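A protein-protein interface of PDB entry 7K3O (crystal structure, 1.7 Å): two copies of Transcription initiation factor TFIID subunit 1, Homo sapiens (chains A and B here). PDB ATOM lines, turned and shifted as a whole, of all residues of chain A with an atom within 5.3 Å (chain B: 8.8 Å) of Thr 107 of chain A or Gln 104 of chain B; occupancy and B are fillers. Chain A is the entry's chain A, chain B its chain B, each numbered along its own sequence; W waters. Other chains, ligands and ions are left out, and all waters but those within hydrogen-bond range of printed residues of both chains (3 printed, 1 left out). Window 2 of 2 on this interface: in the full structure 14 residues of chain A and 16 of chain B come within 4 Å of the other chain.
The side-chain amide oxygen of Asn 100 of chain A is in hydrogen-bond range of the side-chain amide nitrogen of Gln 96 of chain B, at 3.1 Å.
The side-chain hydroxyl (OG1) of Thr 107 of chain B lies within hydrogen-bond range of the side-chain amide oxygen (OE1) of Gln 104 of chain A (2.5 Å).
O of Tyr 103 of chain A sits at hydrogen-bond distance from OG1 of Thr 107 of chain A (3.1 Å).
The side-chain amide oxygen (OD1) of Asn 100 of chain B is in hydrogen-bond range of the side-chain amide nitrogen (NE2) of Gln 96 of chain B (2.9 Å).
The backbone carbonyl oxygen (O) of Tyr 103 of chain B sits at hydrogen-bond distance from the side-chain hydroxyl (OG1) of Thr 107 of chain B (3.1 Å).
Among the printed residues, pairs that only touch across the chains: Asn 100 of chain A with Val 99 of chain B (3.3 Å), Asn 100 of chain A with Tyr 103 of chain B (3.7 Å), Tyr 103 of chain A with Gln 96 of chain B (3.9 Å), Tyr 103 of chain A with Asn 100 of chain B (3.2 Å), Gln 104 of chain A with Tyr 103 of chain B (3.3 Å), Gln 104 of chain A with Gln 104 of chain B (3.7 Å) and Thr 107 of chain A with Gln 104 of chain B (3.6 Å).
Printed residues of chain B within 4 Å of Asn 100 of chain A: Gln 96, Val 99 and Tyr 103.
Printed residues of chain A within 4 Å of Thr 107 of chain B: Gln 104.
Of the printed residues of chain A, Gln 96 of chain B touches Asn 100 and Tyr 103.
Of the printed residues of chain A, Tyr 103 of chain B touches Asn 100 (3.7 Å) and Gln 104 (3.3 Å).
Of the printed residues of chain A, Val 99 of chain B touches Asn 100.
Glu 108 of chain A touches none of the printed residues of chain B.
Leu 71 of chain B touches none of the printed residues of chain A.
The nearest residue of chain B that does not touch Thr 107 of chain A is Asn 100 of chain B (6.5 Å).
The nearest residue of chain A that does not touch Gln 104 of chain B is Tyr 103 of chain A (4.03 Å).
Of the 20 printed residues of chain B, 6 touch a printed residue of chain A.
Hydrophobic or aromatic side chains of chain B within 4 Å of the printed part of chain A: Val 99 and Tyr 103.
Among the printed residues, no Asp or Glu carboxylate lies within 4 Å of a Lys or Arg side-chain nitrogen of the other chain.
Asn 100 of chain A touches Tyr 103 of chain B, and with the chains exchanged Tyr 103 of chain A touches Asn 100 of chain B.
Gln 104 of chain A touches Tyr 103 of chain B, but with the chains exchanged Tyr 103 of chain A does not touch Gln 104 of chain B (4.03 Å).
Gln 104 of chain B touches its own counterpart, Gln 104 of chain A.
Gln 104 of chain A touches Thr 107 of chain B, and with the chains exchanged Thr 107 of chain A touches Gln 104 of chain B.
Positions printed for both chains: 100, 102, 103, 104, 105, 106, 107, 108, 109 and 110.
Water W1 bridges OH of Tyr 103 of chain B and NE2 of Gln 104 of chain A.
Water W2 lies within hydrogen-bond range of OD1 of Asn 100 of chain A (2.8 Å) and OE1 of Gln 96 of chain B (3.3 Å).
Water W3 lies within hydrogen-bond range of the side-chain hydroxyl of Thr 107 of chain A (3.0 Å) and the side-chain amide oxygen of Gln 104 of chain B (3.0 Å).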
ATOM      1  N   ASN A 100       2.879  -0.002  -7.315  1.00  0.00           N
ATOM      2  CA  ASN A 100       1.778   0.677  -6.634  1.00  0.00           C
ATOM      3  C   ASN A 100       0.548  -0.215  -6.558  1.00  0.00           C
ATOM      4  O   ASN A 100      -0.130  -0.252  -5.524  1.00  0.00           O
ATOM      5  CB  ASN A 100       1.438   1.986  -7.338  1.00  0.00           C
ATOM      6  CG  ASN A 100       2.523   3.048  -7.153  1.00  0.00           C
ATOM      7  OD1 ASN A 100       3.439   2.899  -6.331  1.00  0.00           O
ATOM      8  ND2 ASN A 100       2.441   4.105  -7.943  1.00  0.00           N
ATOM      9  N   CYS A 102       0.615  -3.364  -6.475  1.00  0.00           N
ATOM     10  CA  CYS A 102       0.928  -4.434  -5.530  1.00  0.00           C
ATOM     11  C   CYS A 102       0.633  -3.987  -4.097  1.00  0.00           C
ATOM     12  O   CYS A 102      -0.104  -4.657  -3.368  1.00  0.00           O
ATOM     13  CB  CYS A 102       2.398  -4.842  -5.689  1.00  0.00           C
ATOM     14  SG  CYS A 102       2.995  -6.085  -4.519  1.00  0.00           S
ATOM     15  N   TYR A 103       1.142  -2.824  -3.693  1.00  0.00           N
ATOM     16  CA  TYR A 103       0.832  -2.302  -2.359  1.00  0.00           C
ATOM     17  C   TYR A 103      -0.672  -2.155  -2.147  1.00  0.00           C
ATOM     18  O   TYR A 103      -1.194  -2.477  -1.072  1.00  0.00           O
ATOM     19  CB  TYR A 103       1.525  -0.955  -2.145  1.00  0.00           C
ATOM     20  CG  TYR A 103       2.948  -1.065  -1.648  1.00  0.00           C
ATOM     21  CD1 TYR A 103       3.223  -1.242  -0.294  1.00  0.00           C
ATOM     22  CD2 TYR A 103       4.016  -0.978  -2.532  1.00  0.00           C
ATOM     23  CE1 TYR A 103       4.540  -1.345   0.161  1.00  0.00           C
ATOM     24  CE2 TYR A 103       5.334  -1.069  -2.084  1.00  0.00           C
ATOM     25  CZ  TYR A 103       5.582  -1.244  -0.734  1.00  0.00           C
ATOM     26  OH  TYR A 103       6.876  -1.345  -0.263  1.00  0.00           O
ATOM     27  N   GLN A 104      -1.390  -1.654  -3.156  1.00  0.00           N
ATOM     28  CA  GLN A 104      -2.819  -1.435  -2.977  1.00  0.00           C
ATOM     29  C   GLN A 104      -3.561  -2.751  -2.780  1.00  0.00           C
ATOM     30  O   GLN A 104      -4.468  -2.840  -1.945  1.00  0.00           O
ATOM     31  CB  GLN A 104      -3.394  -0.718  -4.196  1.00  0.00           C
ATOM     32  CG  GLN A 104      -4.896  -0.618  -4.162  1.00  0.00           C
ATOM     33  CD  GLN A 104      -5.421   0.236  -5.277  1.00  0.00           C
ATOM     34  OE1 GLN A 104      -5.502   1.454  -5.142  1.00  0.00           O
ATOM     35  NE2 GLN A 104      -5.772  -0.393  -6.402  1.00  0.00           N
ATOM     36  N   THR A 105      -3.171  -3.786  -3.531  1.00  0.00           N
ATOM     37  CA  THR A 105      -3.838  -5.075  -3.393  1.00  0.00           C
ATOM     38  C   THR A 105      -3.501  -5.725  -2.060  1.00  0.00           C
ATOM     39  O   THR A 105      -4.358  -6.356  -1.441  1.00  0.00           O
ATOM     40  CB  THR A 105      -3.463  -5.995  -4.560  1.00  0.00           C
ATOM     41  OG1 THR A 105      -3.668  -5.301  -5.798  1.00  0.00           O
ATOM     42  CG2 THR A 105      -4.339  -7.225  -4.563  1.00  0.00           C
ATOM     43  N   LEU A 106      -2.254  -5.587  -1.602  1.00  0.00           N
ATOM     44  CA  LEU A 106      -1.899  -6.115  -0.288  1.00  0.00           C
ATOM     45  C   LEU A 106      -2.723  -5.462   0.813  1.00  0.00           C
ATOM     46  O   LEU A 106      -3.167  -6.135   1.753  1.00  0.00           O
ATOM     47  CB  LEU A 106      -0.408  -5.903  -0.024  1.00  0.00           C
ATOM     48  CG  LEU A 106       0.561  -6.786  -0.803  1.00  0.00           C
ATOM     49  CD1 LEU A 106       1.976  -6.251  -0.687  1.00  0.00           C
ATOM     50  CD2 LEU A 106       0.497  -8.209  -0.304  1.00  0.00           C
ATOM     51  N   THR A 107      -2.954  -4.152   0.706  1.00  0.00           N
ATOM     52  CA  THR A 107      -3.797  -3.483   1.690  1.00  0.00           C
ATOM     53  C   THR A 107      -5.214  -4.024   1.650  1.00  0.00           C
ATOM     54  O   THR A 107      -5.839  -4.222   2.698  1.00  0.00           O
ATOM     55  CB  THR A 107      -3.775  -1.968   1.455  1.00  0.00           C
ATOM     56  OG1 THR A 107      -2.426  -1.501   1.568  1.00  0.00           O
ATOM     57  CG2 THR A 107      -4.645  -1.247   2.475  1.00  0.00           C
ATOM     58  N   GLU A 108      -5.727  -4.289   0.450  1.00  0.00           N
ATOM     59  CA  GLU A 108      -7.068  -4.843   0.318  1.00  0.00           C
ATOM     60  C   GLU A 108      -7.183  -6.217   0.973  1.00  0.00           C
ATOM     61  O   GLU A 108      -8.246  -6.566   1.492  1.00  0.00           O
ATOM     62  CB  GLU A 108      -7.456  -4.910  -1.165  1.00  0.00           C
ATOM     63  CG  GLU A 108      -7.697  -3.540  -1.803  1.00  0.00           C
ATOM     64  CD  GLU A 108      -7.797  -3.591  -3.327  1.00  0.00           C
ATOM     65  OE1 GLU A 108      -7.997  -2.521  -3.945  1.00  0.00           O
ATOM     66  OE2 GLU A 108      -7.676  -4.695  -3.906  1.00  0.00           O
ATOM     67  N   TYR A 109      -6.108  -7.006   0.967  1.00  0.00           N
ATOM     68  CA  TYR A 109      -6.109  -8.339   1.559  1.00  0.00           C
ATOM     69  C   TYR A 109      -5.477  -8.359   2.950  1.00  0.00           C
ATOM     70  O   TYR A 109      -5.098  -9.434   3.433  1.00  0.00           O
ATOM     71  CB  TYR A 109      -5.369  -9.336   0.660  1.00  0.00           C
ATOM     72  CG  TYR A 109      -5.842  -9.458  -0.780  1.00  0.00           C
ATOM     73  CD1 TYR A 109      -7.084  -8.988  -1.189  1.00  0.00           C
ATOM     74  CD2 TYR A 109      -5.027 -10.059  -1.733  1.00  0.00           C
ATOM     75  CE1 TYR A 109      -7.496  -9.114  -2.516  1.00  0.00           C
ATOM     76  CE2 TYR A 109      -5.429 -10.193  -3.053  1.00  0.00           C
ATOM     77  CZ  TYR A 109      -6.661  -9.718  -3.442  1.00  0.00           C
ATOM     78  OH  TYR A 109      -7.046  -9.852  -4.763  1.00  0.00           O
ATOM     79  N   ASP A 110      -5.350  -7.197   3.595  1.00  0.00           N
ATOM     80  CA  ASP A 110      -4.506  -7.076   4.785  1.00  0.00           C
ATOM     81  C   ASP A 110      -4.947  -8.019   5.899  1.00  0.00           C
ATOM     82  O   ASP A 110      -4.117  -8.707   6.506  1.00  0.00           O
ATOM     83  CB  ASP A 110      -4.500  -5.633   5.278  1.00  0.00           C
ATOM     84  CG  ASP A 110      -3.684  -5.458   6.544  1.00  0.00           C
ATOM     85  OD1 ASP A 110      -2.542  -5.963   6.591  1.00  0.00           O
ATOM     86  OD2 ASP A 110      -4.185  -4.821   7.496  1.00  0.00           O
ATOM     87  N   GLU A 111      -6.244  -8.035   6.214  1.00  0.00           N
ATOM     88  CA  GLU A 111      -6.718  -8.881   7.307  1.00  0.00           C
ATOM     89  C   GLU A 111      -6.435 -10.352   7.022  1.00  0.00           C
ATOM     90  O   GLU A 111      -6.020 -11.098   7.918  1.00  0.00           O
ATOM     91  CB  GLU A 111      -8.212  -8.648   7.545  1.00  0.00           C
ATOM     92  N   ILE B  16      -6.067  15.630  -1.457  1.00  0.00           N
ATOM     93  CA  ILE B  16      -5.259  14.421  -1.364  1.00  0.00           C
ATOM     94  C   ILE B  16      -3.880  14.778  -0.833  1.00  0.00           C
ATOM     95  O   ILE B  16      -3.328  14.079   0.027  1.00  0.00           O
ATOM     96  CB  ILE B  16      -5.168  13.699  -2.719  1.00  0.00           C
ATOM     97  CG1 ILE B  16      -6.565  13.260  -3.162  1.00  0.00           C
ATOM     98  CG2 ILE B  16      -4.245  12.477  -2.598  1.00  0.00           C
ATOM     99  CD1 ILE B  16      -6.603  12.648  -4.547  1.00  0.00           C
ATOM    100  N   LYS B  20      -3.924  13.797   3.191  1.00  0.00           N
ATOM    101  CA  LYS B  20      -3.411  12.441   3.214  1.00  0.00           C
ATOM    102  C   LYS B  20      -1.897  12.414   3.073  1.00  0.00           C
ATOM    103  O   LYS B  20      -1.204  11.905   3.953  1.00  0.00           O
ATOM    104  CB  LYS B  20      -4.061  11.616   2.100  1.00  0.00           C
ATOM    105  CG  LYS B  20      -5.571  11.763   1.995  1.00  0.00           C
ATOM    106  CD  LYS B  20      -6.277  11.050   3.124  1.00  0.00           C
ATOM    107  CE  LYS B  20      -7.783  11.129   2.946  1.00  0.00           C
ATOM    108  NZ  LYS B  20      -8.503  10.674   4.166  1.00  0.00           N
ATOM    109  N   MET B  21      -1.370  12.955   1.978  1.00  0.00           N
ATOM    110  CA  MET B  21       0.052  12.793   1.698  1.00  0.00           C
ATOM    111  C   MET B  21       0.920  13.543   2.699  1.00  0.00           C
ATOM    112  O   MET B  21       1.909  12.998   3.202  1.00  0.00           O
ATOM    113  CB  MET B  21       0.335  13.243   0.274  1.00  0.00           C
ATOM    114  CG  MET B  21      -0.351  12.313  -0.712  1.00  0.00           C
ATOM    115  SD  MET B  21      -0.527  13.015  -2.335  1.00  0.00           S
ATOM    116  CE  MET B  21       1.150  12.859  -2.823  1.00  0.00           C
ATOM    117  N   LEU B  71      -0.500  11.884 -10.807  1.00  0.00           N
ATOM    118  CA  LEU B  71       0.176  10.721 -10.250  1.00  0.00           C
ATOM    119  C   LEU B  71       1.596  10.586 -10.795  1.00  0.00           C
ATOM    120  O   LEU B  71       2.499  10.145 -10.070  1.00  0.00           O
ATOM    121  CB  LEU B  71      -0.651   9.458 -10.522  1.00  0.00           C
ATOM    122  CG  LEU B  71      -0.133   8.118  -9.993  1.00  0.00           C
ATOM    123  CD1 LEU B  71       0.141   8.189  -8.494  1.00  0.00           C
ATOM    124  CD2 LEU B  71      -1.133   7.000 -10.314  1.00  0.00           C
ATOM    125  N   GLN B  96       7.531   6.168  -0.473  1.00  0.00           N
ATOM    126  CA  GLN B  96       6.585   5.179  -0.991  1.00  0.00           C
ATOM    127  C   GLN B  96       5.273   5.212  -0.220  1.00  0.00           C
ATOM    128  O   GLN B  96       4.206   4.972  -0.801  1.00  0.00           O
ATOM    129  CB  GLN B  96       7.181   3.774  -0.975  1.00  0.00           C
ATOM    130  CG  GLN B  96       6.202   2.682  -1.527  1.00  0.00           C
ATOM    131  CD  GLN B  96       5.982   2.735  -3.032  1.00  0.00           C
ATOM    132  OE1 GLN B  96       6.930   2.619  -3.790  1.00  0.00           O
ATOM    133  NE2 GLN B  96       4.717   2.819  -3.471  1.00  0.00           N
ATOM    134  N   GLU B  97       5.324   5.519   1.080  1.00  0.00           N
ATOM    135  CA  GLU B  97       4.082   5.668   1.827  1.00  0.00           C
ATOM    136  C   GLU B  97       3.274   6.849   1.301  1.00  0.00           C
ATOM    137  O   GLU B  97       2.039   6.783   1.232  1.00  0.00           O
ATOM    138  CB  GLU B  97       4.384   5.821   3.316  1.00  0.00           C
ATOM    139  CG  GLU B  97       3.142   5.987   4.170  1.00  0.00           C
ATOM    140  CD  GLU B  97       2.179   4.819   4.056  1.00  0.00           C
ATOM    141  OE1 GLU B  97       2.609   3.706   3.678  1.00  0.00           O
ATOM    142  OE2 GLU B  97       0.982   5.016   4.354  1.00  0.00           O
ATOM    143  N   ILE B  98       3.958   7.935   0.929  1.00  0.00           N
ATOM    144  CA  ILE B  98       3.296   9.085   0.317  1.00  0.00           C
ATOM    145  C   ILE B  98       2.620   8.659  -0.981  1.00  0.00           C
ATOM    146  O   ILE B  98       1.452   8.980  -1.230  1.00  0.00           O
ATOM    147  CB  ILE B  98       4.303  10.226   0.079  1.00  0.00           C
ATOM    148  CG1 ILE B  98       4.743  10.851   1.412  1.00  0.00           C
ATOM    149  CG2 ILE B  98       3.708  11.317  -0.803  1.00  0.00           C
ATOM    150  CD1 ILE B  98       5.882  11.846   1.240  1.00  0.00           C
ATOM    151  N   VAL B  99       3.350   7.919  -1.818  1.00  0.00           N
ATOM    152  CA  VAL B  99       2.780   7.418  -3.066  1.00  0.00           C
ATOM    153  C   VAL B  99       1.595   6.510  -2.778  1.00  0.00           C
ATOM    154  O   VAL B  99       0.547   6.611  -3.426  1.00  0.00           O
ATOM    155  CB  VAL B  99       3.856   6.685  -3.895  1.00  0.00           C
ATOM    156  CG1 VAL B  99       3.208   5.931  -5.081  1.00  0.00           C
ATOM    157  CG2 VAL B  99       4.887   7.660  -4.399  1.00  0.00           C
ATOM    158  N   ASN B 100       1.730   5.619  -1.795  1.00  0.00           N
ATOM    159  CA  ASN B 100       0.660   4.661  -1.546  1.00  0.00           C
ATOM    160  C   ASN B 100      -0.616   5.353  -1.076  1.00  0.00           C
ATOM    161  O   ASN B 100      -1.719   4.993  -1.513  1.00  0.00           O
ATOM    162  CB  ASN B 100       1.104   3.623  -0.517  1.00  0.00           C
ATOM    163  CG  ASN B 100       2.075   2.616  -1.081  1.00  0.00           C
ATOM    164  OD1 ASN B 100       2.150   2.405  -2.295  1.00  0.00           O
ATOM    165  ND2 ASN B 100       2.832   1.968  -0.189  1.00  0.00           N
ATOM    166  N   VAL B 101      -0.499   6.336  -0.175  1.00  0.00           N
ATOM    167  CA  VAL B 101      -1.731   6.984   0.265  1.00  0.00           C
ATOM    168  C   VAL B 101      -2.344   7.769  -0.885  1.00  0.00           C
ATOM    169  O   VAL B 101      -3.571   7.867  -0.989  1.00  0.00           O
ATOM    170  CB  VAL B 101      -1.512   7.866   1.518  1.00  0.00           C
ATOM    171  CG1 VAL B 101      -0.853   7.063   2.616  1.00  0.00           C
ATOM    172  CG2 VAL B 101      -0.700   9.089   1.201  1.00  0.00           C
ATOM    173  N   CYS B 102      -1.518   8.280  -1.797  1.00  0.00           N
ATOM    174  CA  CYS B 102      -2.062   9.011  -2.935  1.00  0.00           C
ATOM    175  C   CYS B 102      -2.777   8.058  -3.895  1.00  0.00           C
ATOM    176  O   CYS B 102      -3.953   8.246  -4.229  1.00  0.00           O
ATOM    177  CB  CYS B 102      -0.929   9.742  -3.659  1.00  0.00           C
ATOM    178  SG  CYS B 102      -1.418  10.494  -5.249  1.00  0.00           S
ATOM    179  N   TYR B 103      -2.090   6.990  -4.294  1.00  0.00           N
ATOM    180  CA  TYR B 103      -2.655   5.996  -5.203  1.00  0.00           C
ATOM    181  C   TYR B 103      -3.933   5.399  -4.638  1.00  0.00           C
ATOM    182  O   TYR B 103      -4.946   5.286  -5.337  1.00  0.00           O
ATOM    183  CB  TYR B 103      -1.596   4.914  -5.439  1.00  0.00           C
ATOM    184  CG  TYR B 103      -1.942   3.902  -6.494  1.00  0.00           C
ATOM    185  CD1 TYR B 103      -2.650   2.753  -6.174  1.00  0.00           C
ATOM    186  CD2 TYR B 103      -1.540   4.088  -7.802  1.00  0.00           C
ATOM    187  CE1 TYR B 103      -2.961   1.817  -7.146  1.00  0.00           C
ATOM    188  CE2 TYR B 103      -1.839   3.146  -8.774  1.00  0.00           C
ATOM    189  CZ  TYR B 103      -2.550   2.029  -8.448  1.00  0.00           C
ATOM    190  OH  TYR B 103      -2.856   1.092  -9.421  1.00  0.00           O
ATOM    191  N   GLN B 104      -3.908   5.021  -3.365  1.00  0.00           N
ATOM    192  CA  GLN B 104      -5.084   4.395  -2.778  1.00  0.00           C
ATOM    193  C   GLN B 104      -6.241   5.380  -2.634  1.00  0.00           C
ATOM    194  O   GLN B 104      -7.403   4.981  -2.789  1.00  0.00           O
ATOM    195  CB  GLN B 104      -4.692   3.711  -1.472  1.00  0.00           C
ATOM    196  CG  GLN B 104      -3.944   2.397  -1.807  1.00  0.00           C
ATOM    197  CD  GLN B 104      -3.040   1.865  -0.711  1.00  0.00           C
ATOM    198  OE1 GLN B 104      -1.891   1.501  -0.973  1.00  0.00           O
ATOM    199  NE2 GLN B 104      -3.560   1.782   0.505  1.00  0.00           N
ATOM    200  N   THR B 105      -5.958   6.657  -2.348  1.00  0.00           N
ATOM    201  CA  THR B 105      -7.044   7.637  -2.285  1.00  0.00           C
ATOM    202  C   THR B 105      -7.629   7.886  -3.673  1.00  0.00           C
ATOM    203  O   THR B 105      -8.849   8.024  -3.823  1.00  0.00           O
ATOM    204  CB  THR B 105      -6.554   8.949  -1.661  1.00  0.00           C
ATOM    205  OG1 THR B 105      -5.991   8.687  -0.369  1.00  0.00           O
ATOM    206  CG2 THR B 105      -7.711   9.930  -1.499  1.00  0.00           C
ATOM    207  N   LEU B 106      -6.775   7.932  -4.703  1.00  0.00           N
ATOM    208  CA  LEU B 106      -7.269   8.071  -6.070  1.00  0.00           C
ATOM    209  C   LEU B 106      -8.174   6.905  -6.441  1.00  0.00           C
ATOM    210  O   LEU B 106      -9.170   7.080  -7.152  1.00  0.00           O
ATOM    211  CB  LEU B 106      -6.102   8.170  -7.052  1.00  0.00           C
ATOM    212  CG  LEU B 106      -5.263   9.444  -7.024  1.00  0.00           C
ATOM    213  CD1 LEU B 106      -4.006   9.249  -7.856  1.00  0.00           C
ATOM    214  CD2 LEU B 106      -6.059  10.633  -7.532  1.00  0.00           C
ATOM    215  N   THR B 107      -7.827   5.699  -5.983  1.00  0.00           N
ATOM    216  CA  THR B 107      -8.699   4.547  -6.187  1.00  0.00           C
ATOM    217  C   THR B 107     -10.021   4.726  -5.453  1.00  0.00           C
ATOM    218  O   THR B 107     -11.086   4.415  -6.000  1.00  0.00           O
ATOM    219  CB  THR B 107      -7.991   3.278  -5.716  1.00  0.00           C
ATOM    220  OG1 THR B 107      -6.819   3.078  -6.513  1.00  0.00           O
ATOM    221  CG2 THR B 107      -8.900   2.062  -5.837  1.00  0.00           C
ATOM    222  N   GLU B 108      -9.970   5.222  -4.211  1.00  0.00           N
ATOM    223  CA  GLU B 108     -11.187   5.515  -3.454  1.00  0.00           C
ATOM    224  C   GLU B 108     -12.099   6.461  -4.222  1.00  0.00           C
ATOM    225  O   GLU B 108     -13.318   6.253  -4.297  1.00  0.00           O
ATOM    226  CB  GLU B 108     -10.821   6.142  -2.106  1.00  0.00           C
ATOM    227  CG  GLU B 108     -11.360   5.410  -0.884  1.00  0.00           C
ATOM    228  CD  GLU B 108     -11.738   6.356   0.246  1.00  0.00           C
ATOM    229  OE1 GLU B 108     -11.021   7.355   0.453  1.00  0.00           O
ATOM    230  OE2 GLU B 108     -12.746   6.092   0.938  1.00  0.00           O
ATOM    231  N   TYR B 109     -11.523   7.524  -4.780  1.00  0.00           N
ATOM    232  CA  TYR B 109     -12.269   8.583  -5.439  1.00  0.00           C
ATOM    233  C   TYR B 109     -12.518   8.293  -6.912  1.00  0.00           C
ATOM    234  O   TYR B 109     -12.842   9.221  -7.662  1.00  0.00           O
ATOM    235  CB  TYR B 109     -11.531   9.920  -5.314  1.00  0.00           C
ATOM    236  CG  TYR B 109     -11.281  10.444  -3.910  1.00  0.00           C
ATOM    237  CD1 TYR B 109     -11.823   9.824  -2.793  1.00  0.00           C
ATOM    238  CD2 TYR B 109     -10.512  11.588  -3.715  1.00  0.00           C
ATOM    239  CE1 TYR B 109     -11.595  10.322  -1.517  1.00  0.00           C
ATOM    240  CE2 TYR B 109     -10.280  12.093  -2.447  1.00  0.00           C
ATOM    241  CZ  TYR B 109     -10.822  11.457  -1.351  1.00  0.00           C
ATOM    242  OH  TYR B 109     -10.587  11.957  -0.088  1.00  0.00           O
ATOM    243  N   ASP B 110     -12.378   7.034  -7.338  1.00  0.00           N
ATOM    244  CA  ASP B 110     -12.337   6.726  -8.766  1.00  0.00           C
ATOM    245  C   ASP B 110     -13.596   7.202  -9.480  1.00  0.00           C
ATOM    246  O   ASP B 110     -13.519   7.877 -10.514  1.00  0.00           O
ATOM    247  CB  ASP B 110     -12.150   5.226  -8.978  1.00  0.00           C
ATOM    248  CG  ASP B 110     -12.198   4.842 -10.439  1.00  0.00           C
ATOM    249  OD1 ASP B 110     -11.468   5.465 -11.234  1.00  0.00           O
ATOM    250  OD2 ASP B 110     -12.970   3.924 -10.798  1.00  0.00           O
ATOM    251  N   LEU B 113     -13.729  11.085  -9.608  1.00  0.00           N
ATOM    252  CA  LEU B 113     -12.710  11.704 -10.450  1.00  0.00           C
ATOM    253  C   LEU B 113     -12.945  11.393 -11.922  1.00  0.00           C
ATOM    254  O   LEU B 113     -12.644  12.219 -12.788  1.00  0.00           O
ATOM    255  CB  LEU B 113     -11.311  11.251 -10.038  1.00  0.00           C
ATOM    256  CG  LEU B 113     -10.790  11.744  -8.694  1.00  0.00           C
ATOM    257  CD1 LEU B 113      -9.690  10.816  -8.186  1.00  0.00           C
ATOM    258  CD2 LEU B 113     -10.307  13.184  -8.808  1.00  0.00           C
HETATM  259  O   HOH W   1      -5.364   0.264  -9.590  1.00  0.00           O
HETATM  260  O   HOH W   2       6.105   3.581  -6.869  1.00  0.00           O
HETATM  261  O   HOH W   3      -0.115   0.260   1.051  1.00  0.00           O
